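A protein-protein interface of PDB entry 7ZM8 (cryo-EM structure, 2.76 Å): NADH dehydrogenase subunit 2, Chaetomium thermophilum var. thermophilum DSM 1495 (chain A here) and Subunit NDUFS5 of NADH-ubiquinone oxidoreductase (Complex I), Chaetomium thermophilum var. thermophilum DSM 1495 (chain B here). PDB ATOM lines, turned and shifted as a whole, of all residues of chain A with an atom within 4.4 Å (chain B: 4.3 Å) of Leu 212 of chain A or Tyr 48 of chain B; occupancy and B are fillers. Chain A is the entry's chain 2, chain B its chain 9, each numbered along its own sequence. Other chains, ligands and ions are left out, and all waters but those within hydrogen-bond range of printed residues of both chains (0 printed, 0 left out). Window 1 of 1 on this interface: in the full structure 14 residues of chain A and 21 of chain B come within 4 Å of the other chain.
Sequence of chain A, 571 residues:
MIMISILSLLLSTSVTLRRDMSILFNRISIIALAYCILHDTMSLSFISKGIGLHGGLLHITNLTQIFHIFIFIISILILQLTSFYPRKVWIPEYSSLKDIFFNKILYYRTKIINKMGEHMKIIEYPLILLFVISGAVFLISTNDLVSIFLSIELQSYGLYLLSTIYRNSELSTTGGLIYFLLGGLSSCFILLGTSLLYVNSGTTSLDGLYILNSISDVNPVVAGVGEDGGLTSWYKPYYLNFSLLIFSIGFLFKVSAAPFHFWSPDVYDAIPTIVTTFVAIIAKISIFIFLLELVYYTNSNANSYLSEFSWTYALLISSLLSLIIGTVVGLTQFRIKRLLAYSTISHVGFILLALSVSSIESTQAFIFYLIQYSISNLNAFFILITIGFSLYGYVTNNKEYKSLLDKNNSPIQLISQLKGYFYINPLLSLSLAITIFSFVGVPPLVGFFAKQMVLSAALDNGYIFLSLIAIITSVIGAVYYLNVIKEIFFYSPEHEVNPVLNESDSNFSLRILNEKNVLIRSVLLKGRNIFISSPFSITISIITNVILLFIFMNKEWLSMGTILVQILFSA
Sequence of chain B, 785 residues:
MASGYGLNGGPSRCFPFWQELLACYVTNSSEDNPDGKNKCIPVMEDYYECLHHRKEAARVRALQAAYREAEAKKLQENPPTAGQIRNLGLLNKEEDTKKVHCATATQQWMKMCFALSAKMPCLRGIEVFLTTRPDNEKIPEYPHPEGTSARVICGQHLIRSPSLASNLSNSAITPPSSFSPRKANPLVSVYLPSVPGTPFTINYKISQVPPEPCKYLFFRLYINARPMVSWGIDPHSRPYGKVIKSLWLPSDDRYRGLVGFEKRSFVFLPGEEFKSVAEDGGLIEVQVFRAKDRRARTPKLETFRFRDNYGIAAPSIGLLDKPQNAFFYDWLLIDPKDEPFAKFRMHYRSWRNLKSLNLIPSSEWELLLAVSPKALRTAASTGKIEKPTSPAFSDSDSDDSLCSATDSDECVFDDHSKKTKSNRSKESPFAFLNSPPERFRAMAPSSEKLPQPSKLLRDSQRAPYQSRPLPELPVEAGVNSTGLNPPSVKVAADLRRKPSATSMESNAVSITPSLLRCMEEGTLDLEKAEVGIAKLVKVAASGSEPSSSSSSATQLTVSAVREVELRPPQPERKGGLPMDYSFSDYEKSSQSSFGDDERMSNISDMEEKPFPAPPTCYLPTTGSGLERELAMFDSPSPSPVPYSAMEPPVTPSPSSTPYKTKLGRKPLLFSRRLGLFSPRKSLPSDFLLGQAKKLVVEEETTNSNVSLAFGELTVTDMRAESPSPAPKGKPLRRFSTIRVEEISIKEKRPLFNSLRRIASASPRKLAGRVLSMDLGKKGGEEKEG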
ATOM      1  N   ASN A 200     -33.412 -24.723  -4.002  1.00  0.00           N
ATOM      2  CA  ASN A 200     -32.170 -24.334  -3.300  1.00  0.00           C
ATOM      3  C   ASN A 200     -31.877 -25.288  -2.162  1.00  0.00           C
ATOM      4  O   ASN A 200     -30.778 -25.218  -1.630  1.00  0.00           O
ATOM      5  CB  ASN A 200     -32.237 -22.882  -2.849  1.00  0.00           C
ATOM      6  CG  ASN A 200     -32.078 -21.893  -3.983  1.00  0.00           C
ATOM      7  OD1 ASN A 200     -31.043 -21.851  -4.636  1.00  0.00           O
ATOM      8  ND2 ASN A 200     -33.095 -21.083  -4.217  1.00  0.00           N
ATOM      9  N   SER A 201     -32.810 -26.165  -1.835  1.00  0.00           N
ATOM     10  CA  SER A 201     -32.672 -27.059  -0.667  1.00  0.00           C
ATOM     11  C   SER A 201     -32.813 -28.526  -1.053  1.00  0.00           C
ATOM     12  O   SER A 201     -32.384 -29.360  -0.270  1.00  0.00           O
ATOM     13  CB  SER A 201     -33.725 -26.699   0.301  1.00  0.00           C
ATOM     14  OG  SER A 201     -35.000 -27.037  -0.203  1.00  0.00           O
ATOM     15  N   GLY A 208     -36.959 -30.484   7.372  1.00  0.00           N
ATOM     16  CA  GLY A 208     -35.619 -30.412   6.767  1.00  0.00           C
ATOM     17  C   GLY A 208     -35.173 -28.980   6.560  1.00  0.00           C
ATOM     18  O   GLY A 208     -34.010 -28.705   6.827  1.00  0.00           O
ATOM     19  N   LEU A 209     -36.067 -28.114   6.097  1.00  0.00           N
ATOM     20  CA  LEU A 209     -35.794 -26.670   5.932  1.00  0.00           C
ATOM     21  C   LEU A 209     -35.514 -26.045   7.293  1.00  0.00           C
ATOM     22  O   LEU A 209     -34.676 -25.138   7.347  1.00  0.00           O
ATOM     23  CB  LEU A 209     -37.044 -26.049   5.315  1.00  0.00           C
ATOM     24  CG  LEU A 209     -37.190 -26.221   3.805  1.00  0.00           C
ATOM     25  CD1 LEU A 209     -38.585 -25.829   3.348  1.00  0.00           C
ATOM     26  CD2 LEU A 209     -36.138 -25.410   3.066  1.00  0.00           C
ATOM     27  N   TYR A 210     -36.233 -26.475   8.332  1.00  0.00           N
ATOM     28  CA  TYR A 210     -36.021 -25.983   9.715  1.00  0.00           C
ATOM     29  C   TYR A 210     -34.626 -26.372  10.202  1.00  0.00           C
ATOM     30  O   TYR A 210     -33.983 -25.540  10.841  1.00  0.00           O
ATOM     31  CB  TYR A 210     -37.111 -26.536  10.635  1.00  0.00           C
ATOM     32  CG  TYR A 210     -38.499 -25.998  10.415  1.00  0.00           C
ATOM     33  CD1 TYR A 210     -38.710 -24.804   9.746  1.00  0.00           C
ATOM     34  CD2 TYR A 210     -39.604 -26.686  10.882  1.00  0.00           C
ATOM     35  CE1 TYR A 210     -39.988 -24.312   9.542  1.00  0.00           C
ATOM     36  CE2 TYR A 210     -40.887 -26.209  10.685  1.00  0.00           C
ATOM     37  CZ  TYR A 210     -41.078 -25.015  10.018  1.00  0.00           C
ATOM     38  OH  TYR A 210     -42.339 -24.535   9.828  1.00  0.00           O
ATOM     39  N   ILE A 211     -34.183 -27.590   9.898  1.00  0.00           N
ATOM     40  CA  ILE A 211     -32.845 -28.087  10.337  1.00  0.00           C
ATOM     41  C   ILE A 211     -31.750 -27.424   9.495  1.00  0.00           C
ATOM     42  O   ILE A 211     -30.687 -27.151  10.040  1.00  0.00           O
ATOM     43  CB  ILE A 211     -32.811 -29.625  10.232  1.00  0.00           C
ATOM     44  CG1 ILE A 211     -33.647 -30.287  11.328  1.00  0.00           C
ATOM     45  CG2 ILE A 211     -31.395 -30.176  10.198  1.00  0.00           C
ATOM     46  CD1 ILE A 211     -33.798 -31.769  11.144  1.00  0.00           C
ATOM     47  N   LEU A 212     -32.007 -27.182   8.213  1.00  0.00           N
ATOM     48  CA  LEU A 212     -31.021 -26.460   7.368  1.00  0.00           C
ATOM     49  C   LEU A 212     -30.860 -25.050   7.933  1.00  0.00           C
ATOM     50  O   LEU A 212     -29.718 -24.587   8.029  1.00  0.00           O
ATOM     51  CB  LEU A 212     -31.501 -26.438   5.913  1.00  0.00           C
ATOM     52  CG  LEU A 212     -31.387 -27.756   5.150  1.00  0.00           C
ATOM     53  CD1 LEU A 212     -32.080 -27.665   3.801  1.00  0.00           C
ATOM     54  CD2 LEU A 212     -29.933 -28.160   4.977  1.00  0.00           C
ATOM     55  N   ASN A 213     -31.968 -24.395   8.275  1.00  0.00           N
ATOM     56  CA  ASN A 213     -31.943 -23.041   8.885  1.00  0.00           C
ATOM     57  C   ASN A 213     -31.265 -23.114  10.255  1.00  0.00           C
ATOM     58  O   ASN A 213     -30.548 -22.168  10.602  1.00  0.00           O
ATOM     59  CB  ASN A 213     -33.359 -22.456   8.946  1.00  0.00           C
ATOM     60  CG  ASN A 213     -33.508 -21.255   9.854  1.00  0.00           C
ATOM     61  OD1 ASN A 213     -32.980 -20.183   9.570  1.00  0.00           O
ATOM     62  ND2 ASN A 213     -34.244 -21.419  10.940  1.00  0.00           N
ATOM     63  N   SER A 214     -31.519 -24.180  11.010  1.00  0.00           N
ATOM     64  CA  SER A 214     -30.951 -24.338  12.373  1.00  0.00           C
ATOM     65  C   SER A 214     -29.426 -24.393  12.308  1.00  0.00           C
ATOM     66  O   SER A 214     -28.784 -23.718  13.119  1.00  0.00           O
ATOM     67  CB  SER A 214     -31.492 -25.594  13.000  1.00  0.00           C
ATOM     68  OG  SER A 214     -31.528 -25.495  14.412  1.00  0.00           O
ATOM     69  N   ILE A 215     -28.875 -25.151  11.366  1.00  0.00           N
ATOM     70  CA  ILE A 215     -27.398 -25.353  11.309  1.00  0.00           C
ATOM     71  C   ILE A 215     -26.743 -24.068  10.795  1.00  0.00           C
ATOM     72  O   ILE A 215     -25.672 -23.719  11.297  1.00  0.00           O
ATOM     73  CB  ILE A 215     -27.064 -26.599  10.462  1.00  0.00           C
ATOM     74  CG1 ILE A 215     -27.684 -27.866  11.054  1.00  0.00           C
ATOM     75  CG2 ILE A 215     -25.571 -26.756  10.249  1.00  0.00           C
ATOM     76  CD1 ILE A 215     -27.772 -29.013  10.079  1.00  0.00           C
ATOM     77  N   SER A 216     -27.389 -23.386   9.854  1.00  0.00           N
ATOM     78  CA  SER A 216     -26.862 -22.114   9.304  1.00  0.00           C
ATOM     79  C   SER A 216     -26.754 -21.028  10.388  1.00  0.00           C
ATOM     80  O   SER A 216     -25.907 -20.140  10.232  1.00  0.00           O
ATOM     81  CB  SER A 216     -27.705 -21.681   8.187  1.00  0.00           C
ATOM     82  OG  SER A 216     -28.905 -21.108   8.677  1.00  0.00           O
ATOM     83  N   TYR A 235     -21.969 -21.847   0.084  1.00  0.00           N
ATOM     84  CA  TYR A 235     -23.445 -21.980   0.072  1.00  0.00           C
ATOM     85  C   TYR A 235     -24.020 -21.259   1.285  1.00  0.00           C
ATOM     86  O   TYR A 235     -24.359 -21.899   2.275  1.00  0.00           O
ATOM     87  CB  TYR A 235     -23.852 -23.450   0.047  1.00  0.00           C
ATOM     88  CG  TYR A 235     -23.397 -24.206  -1.168  1.00  0.00           C
ATOM     89  CD1 TYR A 235     -24.133 -24.169  -2.338  1.00  0.00           C
ATOM     90  CD2 TYR A 235     -22.234 -24.956  -1.144  1.00  0.00           C
ATOM     91  CE1 TYR A 235     -23.719 -24.858  -3.463  1.00  0.00           C
ATOM     92  CE2 TYR A 235     -21.805 -25.643  -2.262  1.00  0.00           C
ATOM     93  CZ  TYR A 235     -22.554 -25.599  -3.421  1.00  0.00           C
ATOM     94  OH  TYR A 235     -22.152 -26.281  -4.523  1.00  0.00           O
ATOM     95  N   TYR A 239     -31.382 -17.814   0.582  1.00  0.00           N
ATOM     96  CA  TYR A 239     -32.648 -18.187  -0.093  1.00  0.00           C
ATOM     97  C   TYR A 239     -33.801 -18.342   0.888  1.00  0.00           C
ATOM     98  O   TYR A 239     -34.910 -18.020   0.485  1.00  0.00           O
ATOM     99  CB  TYR A 239     -32.473 -19.481  -0.891  1.00  0.00           C
ATOM    100  CG  TYR A 239     -32.368 -20.747  -0.079  1.00  0.00           C
ATOM    101  CD1 TYR A 239     -31.159 -21.161   0.452  1.00  0.00           C
ATOM    102  CD2 TYR A 239     -33.477 -21.549   0.139  1.00  0.00           C
ATOM    103  CE1 TYR A 239     -31.058 -22.324   1.193  1.00  0.00           C
ATOM    104  CE2 TYR A 239     -33.395 -22.714   0.881  1.00  0.00           C
ATOM    105  CZ  TYR A 239     -32.179 -23.105   1.408  1.00  0.00           C
ATOM    106  OH  TYR A 239     -32.088 -24.251   2.136  1.00  0.00           O
ATOM    107  N   TRP B  18     -28.031 -36.313   2.580  1.00  0.00           N
ATOM    108  CA  TRP B  18     -29.171 -35.830   3.402  1.00  0.00           C
ATOM    109  C   TRP B  18     -29.361 -36.703   4.641  1.00  0.00           C
ATOM    110  O   TRP B  18     -29.609 -36.152   5.697  1.00  0.00           O
ATOM    111  CB  TRP B  18     -30.434 -35.846   2.529  1.00  0.00           C
ATOM    112  CG  TRP B  18     -31.665 -35.355   3.221  1.00  0.00           C
ATOM    113  CD1 TRP B  18     -32.760 -36.085   3.575  1.00  0.00           C
ATOM    114  CD2 TRP B  18     -31.920 -34.011   3.655  1.00  0.00           C
ATOM    115  NE1 TRP B  18     -33.683 -35.286   4.192  1.00  0.00           N
ATOM    116  CE2 TRP B  18     -33.198 -34.007   4.249  1.00  0.00           C
ATOM    117  CE3 TRP B  18     -31.198 -32.816   3.601  1.00  0.00           C
ATOM    118  CZ2 TRP B  18     -33.760 -32.853   4.790  1.00  0.00           C
ATOM    119  CZ3 TRP B  18     -31.757 -31.676   4.127  1.00  0.00           C
ATOM    120  CH2 TRP B  18     -33.022 -31.696   4.710  1.00  0.00           C
ATOM    121  N   LEU B  21     -26.690 -36.046   6.933  1.00  0.00           N
ATOM    122  CA  LEU B  21     -26.880 -34.731   7.589  1.00  0.00           C
ATOM    123  C   LEU B  21     -27.912 -34.880   8.701  1.00  0.00           C
ATOM    124  O   LEU B  21     -27.681 -34.333   9.789  1.00  0.00           O
ATOM    125  CB  LEU B  21     -27.345 -33.720   6.539  1.00  0.00           C
ATOM    126  CG  LEU B  21     -27.613 -32.305   7.050  1.00  0.00           C
ATOM    127  CD1 LEU B  21     -26.399 -31.752   7.781  1.00  0.00           C
ATOM    128  CD2 LEU B  21     -28.011 -31.391   5.907  1.00  0.00           C
ATOM    129  N   MET B  44     -23.590 -30.405   6.009  1.00  0.00           N
ATOM    130  CA  MET B  44     -24.554 -29.599   5.222  1.00  0.00           C
ATOM    131  C   MET B  44     -23.908 -29.073   3.938  1.00  0.00           C
ATOM    132  O   MET B  44     -24.593 -29.047   2.918  1.00  0.00           O
ATOM    133  CB  MET B  44     -25.065 -28.422   6.050  1.00  0.00           C
ATOM    134  CG  MET B  44     -26.297 -27.762   5.491  1.00  0.00           C
ATOM    135  SD  MET B  44     -26.899 -26.396   6.511  1.00  0.00           S
ATOM    136  CE  MET B  44     -25.465 -25.326   6.506  1.00  0.00           C
ATOM    137  N   GLU B  45     -22.651 -28.640   3.993  1.00  0.00           N
ATOM    138  CA  GLU B  45     -21.926 -28.107   2.814  1.00  0.00           C
ATOM    139  C   GLU B  45     -21.795 -29.213   1.782  1.00  0.00           C
ATOM    140  O   GLU B  45     -21.889 -28.911   0.604  1.00  0.00           O
ATOM    141  CB  GLU B  45     -20.561 -27.586   3.250  1.00  0.00           C
ATOM    142  CG  GLU B  45     -19.952 -26.631   2.243  1.00  0.00           C
ATOM    143  CD  GLU B  45     -18.459 -26.395   2.375  1.00  0.00           C
ATOM    144  OE1 GLU B  45     -17.929 -25.557   1.621  1.00  0.00           O
ATOM    145  OE2 GLU B  45     -17.830 -27.051   3.227  1.00  0.00           O
ATOM    146  N   ASP B  46     -21.557 -30.440   2.226  1.00  0.00           N
ATOM    147  CA  ASP B  46     -21.425 -31.608   1.330  1.00  0.00           C
ATOM    148  C   ASP B  46     -22.754 -31.899   0.641  1.00  0.00           C
ATOM    149  O   ASP B  46     -22.733 -32.360  -0.495  1.00  0.00           O
ATOM    150  CB  ASP B  46     -20.814 -32.782   2.079  1.00  0.00           C
ATOM    151  CG  ASP B  46     -19.312 -32.706   2.229  1.00  0.00           C
ATOM    152  OD1 ASP B  46     -18.763 -31.618   2.029  1.00  0.00           O
ATOM    153  OD2 ASP B  46     -18.707 -33.746   2.525  1.00  0.00           O
ATOM    154  N   TYR B  47     -23.856 -31.607   1.315  1.00  0.00           N
ATOM    155  CA  TYR B  47     -25.187 -31.851   0.736  1.00  0.00           C
ATOM    156  C   TYR B  47     -25.554 -30.689  -0.186  1.00  0.00           C
ATOM    157  O   TYR B  47     -26.116 -30.949  -1.244  1.00  0.00           O
ATOM    158  CB  TYR B  47     -26.203 -32.008   1.864  1.00  0.00           C
ATOM    159  CG  TYR B  47     -27.630 -31.998   1.384  1.00  0.00           C
ATOM    160  CD1 TYR B  47     -28.146 -33.073   0.684  1.00  0.00           C
ATOM    161  CD2 TYR B  47     -28.439 -30.894   1.580  1.00  0.00           C
ATOM    162  CE1 TYR B  47     -29.444 -33.064   0.210  1.00  0.00           C
ATOM    163  CE2 TYR B  47     -29.739 -30.868   1.110  1.00  0.00           C
ATOM    164  CZ  TYR B  47     -30.240 -31.958   0.427  1.00  0.00           C
ATOM    165  OH  TYR B  47     -31.520 -31.946  -0.028  1.00  0.00           O
ATOM    166  N   TYR B  48     -25.223 -29.455   0.190  1.00  0.00           N
ATOM    167  CA  TYR B  48     -25.469 -28.294  -0.698  1.00  0.00           C
ATOM    168  C   TYR B  48     -24.586 -28.434  -1.929  1.00  0.00           C
ATOM    169  O   TYR B  48     -24.967 -27.978  -3.011  1.00  0.00           O
ATOM    170  CB  TYR B  48     -25.287 -26.980   0.049  1.00  0.00           C
ATOM    171  CG  TYR B  48     -26.461 -26.498   0.858  1.00  0.00           C
ATOM    172  CD1 TYR B  48     -27.744 -26.487   0.339  1.00  0.00           C
ATOM    173  CD2 TYR B  48     -26.272 -26.003   2.134  1.00  0.00           C
ATOM    174  CE1 TYR B  48     -28.818 -26.026   1.082  1.00  0.00           C
ATOM    175  CE2 TYR B  48     -27.332 -25.536   2.887  1.00  0.00           C
ATOM    176  CZ  TYR B  48     -28.609 -25.548   2.362  1.00  0.00           C
ATOM    177  OH  TYR B  48     -29.642 -25.083   3.118  1.00  0.00           O
ATOM    178  N   GLU B  49     -23.460 -29.104  -1.763  1.00  0.00           N
ATOM    179  CA  GLU B  49     -22.507 -29.277  -2.875  1.00  0.00           C
ATOM    180  C   GLU B  49     -22.968 -30.431  -3.750  1.00  0.00           C
ATOM    181  O   GLU B  49     -22.788 -30.367  -4.958  1.00  0.00           O
ATOM    182  CB  GLU B  49     -21.128 -29.574  -2.296  1.00  0.00           C
ATOM    183  CG  GLU B  49     -20.090 -30.000  -3.310  1.00  0.00           C
ATOM    184  CD  GLU B  49     -19.725 -28.947  -4.336  1.00  0.00           C
ATOM    185  OE1 GLU B  49     -20.062 -27.777  -4.125  1.00  0.00           O
ATOM    186  OE2 GLU B  49     -19.105 -29.305  -5.342  1.00  0.00           O
ATOM    187  N   CYS B  50     -23.557 -31.464  -3.165  1.00  0.00           N
ATOM    188  CA  CYS B  50     -24.081 -32.566  -3.994  1.00  0.00           C
ATOM    189  C   CYS B  50     -25.166 -32.031  -4.918  1.00  0.00           C
ATOM    190  O   CYS B  50     -25.156 -32.397  -6.065  1.00  0.00           O
ATOM    191  CB  CYS B  50     -24.644 -33.688  -3.131  1.00  0.00           C
ATOM    192  SG  CYS B  50     -25.306 -35.100  -4.058  1.00  0.00           S
ATOM    193  N   LEU B  51     -26.097 -31.236  -4.411  1.00  0.00           N
ATOM    194  CA  LEU B  51     -27.189 -30.677  -5.238  1.00  0.00           C
ATOM    195  C   LEU B  51     -26.691 -29.689  -6.286  1.00  0.00           C
ATOM    196  O   LEU B  51     -27.145 -29.808  -7.428  1.00  0.00           O
ATOM    197  CB  LEU B  51     -28.175 -29.919  -4.350  1.00  0.00           C
ATOM    198  CG  LEU B  51     -28.836 -30.651  -3.190  1.00  0.00           C
ATOM    199  CD1 LEU B  51     -29.458 -29.629  -2.258  1.00  0.00           C
ATOM    200  CD2 LEU B  51     -29.899 -31.615  -3.691  1.00  0.00           C
ATOM    201  N   HIS B  52     -25.807 -28.753  -5.916  1.00  0.00           N
ATOM    202  CA  HIS B  52     -25.437 -27.639  -6.828  1.00  0.00           C
ATOM    203  C   HIS B  52     -24.060 -27.727  -7.483  1.00  0.00           C
ATOM    204  O   HIS B  52     -23.913 -27.043  -8.487  1.00  0.00           O
ATOM    205  CB  HIS B  52     -25.683 -26.308  -6.131  1.00  0.00           C
ATOM    206  CG  HIS B  52     -27.000 -26.205  -5.445  1.00  0.00           C
ATOM    207  ND1 HIS B  52     -28.191 -26.238  -6.130  1.00  0.00           N
ATOM    208  CD2 HIS B  52     -27.314 -26.047  -4.144  1.00  0.00           C
ATOM    209  CE1 HIS B  52     -29.185 -26.125  -5.279  1.00  0.00           C
ATOM    210  NE2 HIS B  52     -28.674 -26.002  -4.059  1.00  0.00           N
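Of chain B, only Leu 21, Met 44 and Tyr 48 come within 4 Å of Leu 212 of chain A. Tyr 48 of chain B touches just these residues of chain A: Asn 200, Leu 212, Tyr 235 and Tyr 239. Of the printed residues of chain A, Tyr 47 of chain B touches Ser 201. Printed residues of chain A within 4 Å of Leu 21 of chain B: Leu 212 (3.9 Å) and Ile 215 (3.8 Å). Of the printed residues of chain B, Tyr 235 of chain A touches Tyr 48 (3.4 Å), Glu 49 (2.6 Å) and His 52 (3.6 Å). Of the printed residues of chain A, His 52 of chain B touches Asn 200 and Tyr 235. Of the printed residues of chain A, Leu 51 of chain B touches Ser 201 (3.5 Å). The nearest printed residue of chain A that does not touch Tyr 48 of chain B is Ser 201 of chain A (4.4 Å). The nearest printed residue of chain B that does not touch Tyr 235 of chain A is Glu 45 of chain B (4.3 Å).
O of Asn 200 of chain A touches CE1 of Tyr 48 of chain B (3.4 Å). Leu 51 of chain B touches Ser 201 of chain A (CD1 to O, 3.5 Å). Trp 18 of chain B touches Gly 208 of chain A. Leu 21 of chain B touches Leu 212 of chain A (CD2 to CD2, 3.9 Å). Leu 212 of chain A touches Tyr 48 of chain B (CD2 to OH, 3.6 Å). Ile 215 of chain A touches Leu 21 of chain B (CD1 to CD1, 3.8 Å). CB of Ile 215 of chain A touches SD of Met 44 of chain B, at 3.96 Å. Tyr 235 of chain A touches Tyr 48 of chain B (CE1 to O, 3.4 Å). His 52 of chain B touches Tyr 235 of chain A.
Of the 13 printed residues of chain A, 7 touch a printed residue of chain B. Hydrophobic or aromatic side chains of chain A within 4 Å of the printed part of chain B: Leu 212, Ile 215, Tyr 235 and Tyr 239. Of the 11 printed residues of chain B, 8 touch a printed residue of chain A. Printed residues of chain B that touch a printed residue of chain A: Trp 18, Leu 21, Met 44, Tyr 47, Tyr 48, Glu 49, Leu 51 and His 52. Hydrophobic or aromatic side chains of chain B within 4 Å of the printed part of chain A: Trp 18, Leu 21, Met 44, Tyr 47, Tyr 48, Leu 51 and His 52. Among the printed residues, 14 pairs touch across the chains.
OH of Tyr 235 of chain A lies within hydrogen-bond range of OE1 of Glu 49 of chain B (2.6 Å). The side-chain sulfur (SD) of Met 44 of chain B lies close to the backbone carbonyl oxygen (O) of Leu 212 of chain A. OH of Tyr 239 of chain A is in hydrogen-bond range of OH of Tyr 48 of chain B (2.8 Å). O of Ser 201 of chain A sits at hydrogen-bond distance from OH of Tyr 47 of chain B. O of Asn 200 of chain A sits at hydrogen-bond distance from NE2 of His 52 of chain B (3.3 Å).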
